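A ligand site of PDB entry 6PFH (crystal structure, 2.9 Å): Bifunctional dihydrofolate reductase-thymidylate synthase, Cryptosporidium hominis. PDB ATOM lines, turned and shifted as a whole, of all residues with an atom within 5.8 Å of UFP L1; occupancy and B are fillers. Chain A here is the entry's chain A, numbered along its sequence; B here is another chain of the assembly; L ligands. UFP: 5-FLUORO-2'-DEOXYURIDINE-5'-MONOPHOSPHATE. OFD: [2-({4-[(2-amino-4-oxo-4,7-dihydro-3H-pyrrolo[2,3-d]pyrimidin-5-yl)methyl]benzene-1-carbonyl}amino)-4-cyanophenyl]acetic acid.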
ATOM      1  N   ASN A 256      -8.641  22.926  31.107  1.00  0.00           N
ATOM      2  CA  ASN A 256      -8.063  21.757  30.442  1.00  0.00           C
ATOM      3  C   ASN A 256      -8.348  20.517  31.281  1.00  0.00           C
ATOM      4  O   ASN A 256      -9.101  20.568  32.257  1.00  0.00           O
ATOM      5  CB  ASN A 256      -6.561  21.954  30.204  1.00  0.00           C
ATOM      6  CG  ASN A 256      -5.815  22.315  31.464  1.00  0.00           C
ATOM      7  OD1 ASN A 256      -5.463  21.443  32.260  1.00  0.00           O
ATOM      8  ND2 ASN A 256      -5.548  23.600  31.649  1.00  0.00           N
ATOM      9  N   ARG A 257      -7.733  19.400  30.894  1.00  0.00           N
ATOM     10  CA  ARG A 257      -8.015  18.124  31.549  1.00  0.00           C
ATOM     11  C   ARG A 257      -7.598  18.126  33.017  1.00  0.00           C
ATOM     12  O   ARG A 257      -8.157  17.368  33.816  1.00  0.00           O
ATOM     13  CB  ARG A 257      -7.304  16.989  30.804  1.00  0.00           C
ATOM     14  CG  ARG A 257      -5.805  17.196  30.676  1.00  0.00           C
ATOM     15  CD  ARG A 257      -5.099  15.960  30.150  1.00  0.00           C
ATOM     16  NE  ARG A 257      -3.653  16.154  30.215  1.00  0.00           N
ATOM     17  CZ  ARG A 257      -2.919  15.899  31.284  1.00  0.00           C
ATOM     18  NH1 ARG A 257      -3.494  15.427  32.381  1.00  0.00           N
ATOM     19  NH2 ARG A 257      -1.606  16.094  31.264  1.00  0.00           N
ATOM     20  N   GLU A 294      16.097  11.136  30.728  1.00  0.00           N
ATOM     21  CA  GLU A 294      14.853  10.905  30.011  1.00  0.00           C
ATOM     22  C   GLU A 294      15.109  10.616  28.537  1.00  0.00           C
ATOM     23  O   GLU A 294      14.445   9.772  27.939  1.00  0.00           O
ATOM     24  CB  GLU A 294      13.921  12.112  30.149  1.00  0.00           C
ATOM     25  CG  GLU A 294      12.579  11.953  29.442  1.00  0.00           C
ATOM     26  CD  GLU A 294      11.905  13.281  29.163  1.00  0.00           C
ATOM     27  OE1 GLU A 294      12.617  14.255  28.861  1.00  0.00           O
ATOM     28  OE2 GLU A 294      10.659  13.346  29.246  1.00  0.00           O
ATOM     29  N   TRP A 316       8.300  11.757  35.398  1.00  0.00           N
ATOM     30  CA  TRP A 316       7.185  10.925  34.951  1.00  0.00           C
ATOM     31  C   TRP A 316       6.488  10.208  36.092  1.00  0.00           C
ATOM     32  O   TRP A 316       5.816   9.201  35.864  1.00  0.00           O
ATOM     33  CB  TRP A 316       7.650   9.910  33.907  1.00  0.00           C
ATOM     34  CG  TRP A 316       7.922  10.497  32.554  1.00  0.00           C
ATOM     35  CD1 TRP A 316       9.130  10.836  32.037  1.00  0.00           C
ATOM     36  CD2 TRP A 316       6.946  10.809  31.544  1.00  0.00           C
ATOM     37  NE1 TRP A 316       8.972  11.341  30.767  1.00  0.00           N
ATOM     38  CE2 TRP A 316       7.640  11.343  30.446  1.00  0.00           C
ATOM     39  CE3 TRP A 316       5.555  10.700  31.473  1.00  0.00           C
ATOM     40  CZ2 TRP A 316       6.999  11.751  29.277  1.00  0.00           C
ATOM     41  CZ3 TRP A 316       4.912  11.112  30.318  1.00  0.00           C
ATOM     42  CH2 TRP A 316       5.630  11.634  29.236  1.00  0.00           C
ATOM     43  N   TYR A 342       6.735   7.684  23.763  1.00  0.00           N
ATOM     44  CA  TYR A 342       7.845   8.127  22.916  1.00  0.00           C
ATOM     45  C   TYR A 342       8.859   7.026  22.640  1.00  0.00           C
ATOM     46  O   TYR A 342       9.136   6.699  21.481  1.00  0.00           O
ATOM     47  CB  TYR A 342       8.540   9.337  23.555  1.00  0.00           C
ATOM     48  CG  TYR A 342       7.623  10.443  24.022  1.00  0.00           C
ATOM     49  CD1 TYR A 342       7.116  11.377  23.130  1.00  0.00           C
ATOM     50  CD2 TYR A 342       7.242  10.538  25.353  1.00  0.00           C
ATOM     51  CE1 TYR A 342       6.284  12.397  23.559  1.00  0.00           C
ATOM     52  CE2 TYR A 342       6.405  11.557  25.789  1.00  0.00           C
ATOM     53  CZ  TYR A 342       5.926  12.478  24.876  1.00  0.00           C
ATOM     54  OH  TYR A 342       5.085  13.489  25.307  1.00  0.00           O
ATOM     55  N   LEU A 399       0.015   9.231  28.557  1.00  0.00           N
ATOM     56  CA  LEU A 399      -0.092  10.606  28.095  1.00  0.00           C
ATOM     57  C   LEU A 399       0.247  10.650  26.615  1.00  0.00           C
ATOM     58  O   LEU A 399       1.277  10.114  26.206  1.00  0.00           O
ATOM     59  CB  LEU A 399       0.838  11.517  28.899  1.00  0.00           C
ATOM     60  CG  LEU A 399       0.614  13.025  28.734  1.00  0.00           C
ATOM     61  CD1 LEU A 399      -0.746  13.406  29.300  1.00  0.00           C
ATOM     62  CD2 LEU A 399       1.723  13.820  29.407  1.00  0.00           C
ATOM     63  N   PRO A 400      -0.604  11.252  25.781  1.00  0.00           N
ATOM     64  CA  PRO A 400      -0.286  11.349  24.354  1.00  0.00           C
ATOM     65  C   PRO A 400       0.975  12.157  24.135  1.00  0.00           C
ATOM     66  O   PRO A 400       1.349  12.987  24.984  1.00  0.00           O
ATOM     67  CB  PRO A 400      -1.522  12.056  23.773  1.00  0.00           C
ATOM     68  CG  PRO A 400      -2.614  11.759  24.738  1.00  0.00           C
ATOM     69  CD  PRO A 400      -1.952  11.751  26.085  1.00  0.00           C
ATOM     70  N   CYS A 402       3.623  14.912  23.321  1.00  0.00           N
ATOM     71  CA  CYS A 402       3.645  16.369  23.211  1.00  0.00           C
ATOM     72  C   CYS A 402       4.591  16.825  22.109  1.00  0.00           C
ATOM     73  O   CYS A 402       4.187  17.570  21.212  1.00  0.00           O
ATOM     74  CB  CYS A 402       4.043  16.985  24.561  1.00  0.00           C
ATOM     75  SG  CYS A 402       2.819  16.696  25.850  1.00  0.00           S
ATOM     76  N   HIS A 403       5.850  16.403  22.173  1.00  0.00           N
ATOM     77  CA  HIS A 403       6.759  16.530  21.023  1.00  0.00           C
ATOM     78  C   HIS A 403       6.388  15.420  20.055  1.00  0.00           C
ATOM     79  O   HIS A 403       6.853  14.279  20.168  1.00  0.00           O
ATOM     80  CB  HIS A 403       8.221  16.503  21.446  1.00  0.00           C
ATOM     81  CG  HIS A 403       8.545  15.503  22.512  1.00  0.00           C
ATOM     82  ND1 HIS A 403       9.373  14.420  22.288  1.00  0.00           N
ATOM     83  CD2 HIS A 403       8.183  15.431  23.815  1.00  0.00           C
ATOM     84  CE1 HIS A 403       9.492  13.721  23.392  1.00  0.00           C
ATOM     85  NE2 HIS A 403       8.785  14.304  24.344  1.00  0.00           N
ATOM     86  N   GLN A 422       5.468  20.555  18.320  1.00  0.00           N
ATOM     87  CA  GLN A 422       4.971  20.272  19.668  1.00  0.00           C
ATOM     88  C   GLN A 422       3.517  20.714  19.730  1.00  0.00           C
ATOM     89  O   GLN A 422       3.215  21.899  19.553  1.00  0.00           O
ATOM     90  CB  GLN A 422       5.824  20.997  20.708  1.00  0.00           C
ATOM     91  CG  GLN A 422       5.603  20.555  22.140  1.00  0.00           C
ATOM     92  CD  GLN A 422       6.646  21.117  23.083  1.00  0.00           C
ATOM     93  OE1 GLN A 422       7.532  21.870  22.664  1.00  0.00           O
ATOM     94  NE2 GLN A 422       6.541  20.774  24.361  1.00  0.00           N
ATOM     95  N   ARG A 423       2.608  19.758  19.966  1.00  0.00           N
ATOM     96  CA  ARG A 423       1.187  20.072  19.959  1.00  0.00           C
ATOM     97  C   ARG A 423       0.792  20.866  21.203  1.00  0.00           C
ATOM     98  O   ARG A 423      -0.071  21.748  21.127  1.00  0.00           O
ATOM     99  CB  ARG A 423       0.359  18.790  19.870  1.00  0.00           C
ATOM    100  CG  ARG A 423       0.548  17.846  21.045  1.00  0.00           C
ATOM    101  CD  ARG A 423      -0.606  16.861  21.188  1.00  0.00           C
ATOM    102  NE  ARG A 423      -0.463  16.051  22.382  1.00  0.00           N
ATOM    103  CZ  ARG A 423      -0.899  16.410  23.593  1.00  0.00           C
ATOM    104  NH1 ARG A 423      -1.522  17.568  23.757  1.00  0.00           N
ATOM    105  NH2 ARG A 423      -0.724  15.609  24.629  1.00  0.00           N
ATOM    106  N   SER A 424       1.399  20.559  22.336  1.00  0.00           N
ATOM    107  CA  SER A 424       1.089  21.206  23.602  1.00  0.00           C
ATOM    108  C   SER A 424       2.389  21.484  24.327  1.00  0.00           C
ATOM    109  O   SER A 424       3.249  20.598  24.427  1.00  0.00           O
ATOM    110  CB  SER A 424       0.158  20.331  24.454  1.00  0.00           C
ATOM    111  OG  SER A 424      -0.107  20.940  25.704  1.00  0.00           O
ATOM    112  N   CYS A 425       2.540  22.701  24.837  1.00  0.00           N
ATOM    113  CA  CYS A 425       3.810  23.162  25.384  1.00  0.00           C
ATOM    114  C   CYS A 425       3.587  23.846  26.721  1.00  0.00           C
ATOM    115  O   CYS A 425       3.099  24.978  26.775  1.00  0.00           O
ATOM    116  CB  CYS A 425       4.498  24.115  24.408  1.00  0.00           C
ATOM    117  SG  CYS A 425       6.118  24.665  24.955  1.00  0.00           S
ATOM    118  N   ASP A 426       3.961  23.155  27.800  1.00  0.00           N
ATOM    119  CA  ASP A 426       4.043  23.766  29.125  1.00  0.00           C
ATOM    120  C   ASP A 426       5.287  24.638  29.169  1.00  0.00           C
ATOM    121  O   ASP A 426       6.402  24.131  29.299  1.00  0.00           O
ATOM    122  CB  ASP A 426       4.075  22.680  30.202  1.00  0.00           C
ATOM    123  CG  ASP A 426       4.114  23.247  31.612  1.00  0.00           C
ATOM    124  OD1 ASP A 426       4.098  24.484  31.773  1.00  0.00           O
ATOM    125  OD2 ASP A 426       4.147  22.437  32.566  1.00  0.00           O
ATOM    126  N   LEU A 427       5.102  25.949  29.052  1.00  0.00           N
ATOM    127  CA  LEU A 427       6.246  26.855  28.982  1.00  0.00           C
ATOM    128  C   LEU A 427       7.007  26.933  30.293  1.00  0.00           C
ATOM    129  O   LEU A 427       8.169  27.370  30.296  1.00  0.00           O
ATOM    130  CB  LEU A 427       5.785  28.256  28.569  1.00  0.00           C
ATOM    131  CG  LEU A 427       5.320  28.431  27.120  1.00  0.00           C
ATOM    132  CD1 LEU A 427       4.832  29.842  26.890  1.00  0.00           C
ATOM    133  CD2 LEU A 427       6.461  28.107  26.175  1.00  0.00           C
ATOM    134  N   GLY A 430       7.864  21.927  30.713  1.00  0.00           N
ATOM    135  CA  GLY A 430       8.190  21.063  29.588  1.00  0.00           C
ATOM    136  C   GLY A 430       9.036  21.733  28.529  1.00  0.00           C
ATOM    137  O   GLY A 430       9.914  21.107  27.935  1.00  0.00           O
ATOM    138  N   SER A 431       8.795  23.029  28.293  1.00  0.00           N
ATOM    139  CA  SER A 431       9.468  23.707  27.185  1.00  0.00           C
ATOM    140  C   SER A 431      10.980  23.755  27.337  1.00  0.00           C
ATOM    141  O   SER A 431      11.679  23.397  26.386  1.00  0.00           O
ATOM    142  CB  SER A 431       8.876  25.110  27.000  1.00  0.00           C
ATOM    143  OG  SER A 431       9.346  25.694  25.798  1.00  0.00           O
ATOM    144  N   ASN A 434      12.208  20.336  26.647  1.00  0.00           N
ATOM    145  CA  ASN A 434      12.115  19.948  25.239  1.00  0.00           C
ATOM    146  C   ASN A 434      13.217  20.578  24.407  1.00  0.00           C
ATOM    147  O   ASN A 434      13.780  19.939  23.519  1.00  0.00           O
ATOM    148  CB  ASN A 434      10.747  20.324  24.677  1.00  0.00           C
ATOM    149  CG  ASN A 434       9.642  19.420  25.158  1.00  0.00           C
ATOM    150  OD1 ASN A 434       8.628  19.876  25.674  1.00  0.00           O
ATOM    151  ND2 ASN A 434       9.838  18.111  25.002  1.00  0.00           N
ATOM    152  N   HIS A 464       1.152  27.441  26.256  1.00  0.00           N
ATOM    153  CA  HIS A 464       0.355  27.873  27.391  1.00  0.00           C
ATOM    154  C   HIS A 464       1.213  28.034  28.637  1.00  0.00           C
ATOM    155  O   HIS A 464       2.315  27.483  28.742  1.00  0.00           O
ATOM    156  CB  HIS A 464      -0.797  26.898  27.661  1.00  0.00           C
ATOM    157  CG  HIS A 464      -0.358  25.467  27.722  1.00  0.00           C
ATOM    158  ND1 HIS A 464       0.135  24.892  28.870  1.00  0.00           N
ATOM    159  CD2 HIS A 464      -0.320  24.500  26.766  1.00  0.00           C
ATOM    160  CE1 HIS A 464       0.449  23.629  28.627  1.00  0.00           C
ATOM    161  NE2 HIS A 464       0.169  23.369  27.361  1.00  0.00           N
ATOM    162  N   TYR A 466       0.609  27.698  32.843  1.00  0.00           N
ATOM    163  CA  TYR A 466      -0.300  27.312  33.918  1.00  0.00           C
ATOM    164  C   TYR A 466      -0.410  28.437  34.933  1.00  0.00           C
ATOM    165  O   TYR A 466       0.571  29.116  35.244  1.00  0.00           O
ATOM    166  CB  TYR A 466       0.177  26.020  34.584  1.00  0.00           C
ATOM    167  CG  TYR A 466      -0.139  24.787  33.768  1.00  0.00           C
ATOM    168  CD1 TYR A 466       0.747  24.324  32.805  1.00  0.00           C
ATOM    169  CD2 TYR A 466      -1.324  24.089  33.954  1.00  0.00           C
ATOM    170  CE1 TYR A 466       0.457  23.198  32.047  1.00  0.00           C
ATOM    171  CE2 TYR A 466      -1.627  22.966  33.200  1.00  0.00           C
ATOM    172  CZ  TYR A 466      -0.729  22.525  32.254  1.00  0.00           C
ATOM    173  OH  TYR A 466      -1.034  21.407  31.513  1.00  0.00           O
ATOM    174  N   ASP B 381      -9.761  20.736  24.145  1.00  0.00           N
ATOM    175  CA  ASP B 381      -8.808  19.644  24.144  1.00  0.00           C
ATOM    176  C   ASP B 381      -7.577  20.028  23.325  1.00  0.00           C
ATOM    177  O   ASP B 381      -7.691  20.715  22.302  1.00  0.00           O
ATOM    178  CB  ASP B 381      -9.459  18.381  23.577  1.00  0.00           C
ATOM    179  CG  ASP B 381      -8.559  17.154  23.662  1.00  0.00           C
ATOM    180  OD1 ASP B 381      -8.034  16.865  24.759  1.00  0.00           O
ATOM    181  OD2 ASP B 381      -8.394  16.483  22.630  1.00  0.00           O
ATOM    182  N   ARG B 382      -6.402  19.586  23.770  1.00  0.00           N
ATOM    183  CA  ARG B 382      -5.146  19.925  23.131  1.00  0.00           C
ATOM    184  C   ARG B 382      -4.653  18.835  22.179  1.00  0.00           C
ATOM    185  O   ARG B 382      -3.456  18.780  21.871  1.00  0.00           O
ATOM    186  CB  ARG B 382      -4.071  20.206  24.181  1.00  0.00           C
ATOM    187  CG  ARG B 382      -4.420  21.211  25.266  1.00  0.00           C
ATOM    188  CD  ARG B 382      -3.147  21.553  26.017  1.00  0.00           C
ATOM    189  NE  ARG B 382      -3.339  22.262  27.281  1.00  0.00           N
ATOM    190  CZ  ARG B 382      -3.240  21.704  28.483  1.00  0.00           C
ATOM    191  NH1 ARG B 382      -2.958  20.406  28.606  1.00  0.00           N
ATOM    192  NH2 ARG B 382      -3.400  22.442  29.568  1.00  0.00           N
ATOM    193  N   ARG B 383      -5.550  17.958  21.712  1.00  0.00           N
ATOM    194  CA  ARG B 383      -5.138  16.782  20.959  1.00  0.00           C
ATOM    195  C   ARG B 383      -5.921  16.625  19.657  1.00  0.00           C
ATOM    196  O   ARG B 383      -6.143  15.511  19.189  1.00  0.00           O
ATOM    197  CB  ARG B 383      -5.279  15.519  21.817  1.00  0.00           C
ATOM    198  CG  ARG B 383      -4.496  15.581  23.115  1.00  0.00           C
ATOM    199  CD  ARG B 383      -4.990  14.544  24.103  1.00  0.00           C
ATOM    200  NE  ARG B 383      -4.314  14.653  25.380  1.00  0.00           N
ATOM    201  CZ  ARG B 383      -4.612  13.920  26.461  1.00  0.00           C
ATOM    202  NH1 ARG B 383      -5.586  13.034  26.409  1.00  0.00           N
ATOM    203  NH2 ARG B 383      -3.932  14.091  27.587  1.00  0.00           N
HETATM  204  N1  UFP L   1       4.308  18.762  28.280  1.00  0.00           N
HETATM  205  C2  UFP L   1       5.213  19.468  27.539  1.00  0.00           C
HETATM  206  N3  UFP L   1       6.298  18.858  27.030  1.00  0.00           N
HETATM  207  C4  UFP L   1       6.526  17.549  27.238  1.00  0.00           C
HETATM  208  C5  UFP L   1       5.602  16.806  28.005  1.00  0.00           C
HETATM  209  C6  UFP L   1       4.524  17.440  28.514  1.00  0.00           C
HETATM  210  O2  UFP L   1       5.090  20.660  27.285  1.00  0.00           O
HETATM  211  O4  UFP L   1       7.522  17.008  26.772  1.00  0.00           O
HETATM  212  F5  UFP L   1       5.792  15.491  28.246  1.00  0.00           F
HETATM  213  C1' UFP L   1       3.082  19.311  28.893  1.00  0.00           C
HETATM  214  C2' UFP L   1       2.171  20.131  27.948  1.00  0.00           C
HETATM  215  C3' UFP L   1       0.831  20.042  28.694  1.00  0.00           C
HETATM  216  C4' UFP L   1       0.829  18.593  29.202  1.00  0.00           C
HETATM  217  O3' UFP L   1       0.796  20.941  29.804  1.00  0.00           O
HETATM  218  O4' UFP L   1       2.223  18.197  29.280  1.00  0.00           O
HETATM  219  C5' UFP L   1       0.043  17.691  28.252  1.00  0.00           C
HETATM  220  O5' UFP L   1      -1.330  17.687  28.649  1.00  0.00           O
HETATM  221  P   UFP L   1      -2.231  17.576  27.318  1.00  0.00           P
HETATM  222  O1P UFP L   1      -3.741  17.965  27.678  1.00  0.00           O
HETATM  223  O2P UFP L   1      -1.720  18.519  26.298  1.00  0.00           O
HETATM  224  O3P UFP L   1      -2.171  16.078  26.741  1.00  0.00           O
HETATM  225  O1  OFD L   2       5.897  19.311  31.604  1.00  0.00           O
HETATM  226  C1  OFD L   2       2.579  18.336  32.334  1.00  0.00           C
HETATM  227  O2  OFD L   2       9.098  18.769  37.003  1.00  0.00           O
HETATM  228  C2  OFD L   2       3.771  16.451  31.931  1.00  0.00           C
HETATM  229  C3  OFD L   2       4.942  17.125  31.698  1.00  0.00           C
HETATM  230  C4  OFD L   2       4.903  18.601  31.798  1.00  0.00           C
HETATM  231  C5  OFD L   2       5.941  16.149  31.397  1.00  0.00           C
HETATM  232  C6  OFD L   2       5.335  14.911  31.469  1.00  0.00           C
HETATM  233  C7  OFD L   2       7.388  16.389  31.087  1.00  0.00           C
HETATM  234  C8  OFD L   2       7.991  17.017  32.317  1.00  0.00           C
HETATM  235  C9  OFD L   2       7.504  16.659  33.594  1.00  0.00           C
HETATM  236  C10 OFD L   2       8.051  17.250  34.751  1.00  0.00           C
HETATM  237  C11 OFD L   2       9.083  18.204  34.643  1.00  0.00           C
HETATM  238  C12 OFD L   2       9.561  18.573  33.376  1.00  0.00           C
HETATM  239  O3  OFD L   2      13.540  16.163  38.124  1.00  0.00           O
HETATM  240  C13 OFD L   2       9.020  17.984  32.212  1.00  0.00           C
HETATM  241  C14 OFD L   2       9.631  18.831  35.894  1.00  0.00           C
HETATM  242  C15 OFD L   2      11.550  20.186  36.707  1.00  0.00           C
HETATM  243  C16 OFD L   2      12.133  19.553  37.831  1.00  0.00           C
HETATM  244  C17 OFD L   2      12.846  20.315  38.781  1.00  0.00           C
HETATM  245  C18 OFD L   2      12.987  21.710  38.615  1.00  0.00           C
HETATM  246  C19 OFD L   2      12.404  22.343  37.490  1.00  0.00           C
HETATM  247  C20 OFD L   2      11.685  21.579  36.548  1.00  0.00           C
HETATM  248  C21 OFD L   2      12.549  23.823  37.302  1.00  0.00           C
HETATM  249  C22 OFD L   2      12.000  18.065  38.040  1.00  0.00           C
HETATM  250  C23 OFD L   2      13.325  17.360  37.943  1.00  0.00           C
HETATM  251  N1  OFD L   2       3.719  19.125  32.115  1.00  0.00           N
HETATM  252  N2  OFD L   2       2.546  17.031  32.258  1.00  0.00           N
HETATM  253  N3  OFD L   2       4.001  15.110  31.793  1.00  0.00           N
HETATM  254  N4  OFD L   2       1.387  19.106  32.660  1.00  0.00           N
HETATM  255  N5  OFD L   2      10.789  19.461  35.690  1.00  0.00           N
HETATM  256  N6  OFD L   2      12.649  24.966  37.151  1.00  0.00           N
HETATM  257  O4  OFD L   2      14.301  18.253  37.634  1.00  0.00           O
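OH of Tyr 466 is in hydrogen-bond range of NH2 of Arg 382 of chain B, 3.2 Å away. The backbone NH of Arg 383 of chain B lies close to the side-chain carboxylate of Asp 381 of chain B (3.3 Å). The side-chain amide oxygen of Asn 434 sits at hydrogen-bond distance from the side-chain amide nitrogen of Gln 422 (2.6 Å). OD1 of Asn 434 lies close to O of Gly 430 (2.9 Å). OG of Ser 424 lies within hydrogen-bond range of NE2 of His 464 (3.0 Å). The backbone carbonyl oxygen (O) of His 464 is in hydrogen-bond range of the backbone NH (N) of Leu 427, 3.2 Å away. NE2 of Gln 422 sits close to O of Ser 424 (3.3 Å). NE1 of Trp 316 is in hydrogen-bond range of OE2 of Glu 294, 3.0 Å away.
O3' of UFP L1 is in hydrogen-bond range of OH of Tyr 466 (2.5 Å). The guanidinium group of Arg 423 is in salt-bridge range of an oxygen (O3P) of UFP L1 (2.6 Å). The guanidinium group (NH1) of Arg 382 of chain B is in salt-bridge range of an oxygen (O1P) of UFP L1. O3P of UFP L1 lies within salt-bridge range of NH2 of Arg 383 of chain B (2.8 Å). The backbone NH (N) of Asp 426 is in hydrogen-bond range of an oxygen (O2) of UFP L1, at 2.8 Å. OD1 of Asn 434 sits at hydrogen-bond distance from N3 of UFP L1, 2.9 Å away. The side-chain hydroxyl (OG) of Ser 424 lies within hydrogen-bond range of an oxygen (O2P) of UFP L1. The guanidinium group of Arg 257 is in salt-bridge range of an oxygen (O1P) of UFP L1 (3.1 Å). SG of Cys 402 sits close to O4' of UFP L1, 3.8 Å away. NE2 of Gln 422 is in hydrogen-bond range of O2 of UFP L1 (3.3 Å). N1 of OFD L2 lies within hydrogen-bond range of OD2 of Asp 426 (3.4 Å). The backbone NH (N) of Gly 430 is in hydrogen-bond range of an oxygen (O1) of OFD L2 (3.4 Å).
N1 of OFD L2 lies close to O4' of UFP L1 (3.3 Å).
Merely in contact with UFP L1: His 464, Cys 425, His 403, Tyr 342, Gly 430, Leu 399 and Trp 316. Hydrophobic or aromatic side chains that line UFP L1: Trp 316, Leu 399, His 403, His 464 and Tyr 466. Within 4 Å of UFP L1: Arg 257, Trp 316, Tyr 342, Leu 399, Cys 402, His 403, Gln 422, Arg 423, Ser 424, Cys 425, Asp 426, Gly 430, Asn 434, His 464, Tyr 466, Arg 382 of chain B and Arg 383 of chain B.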
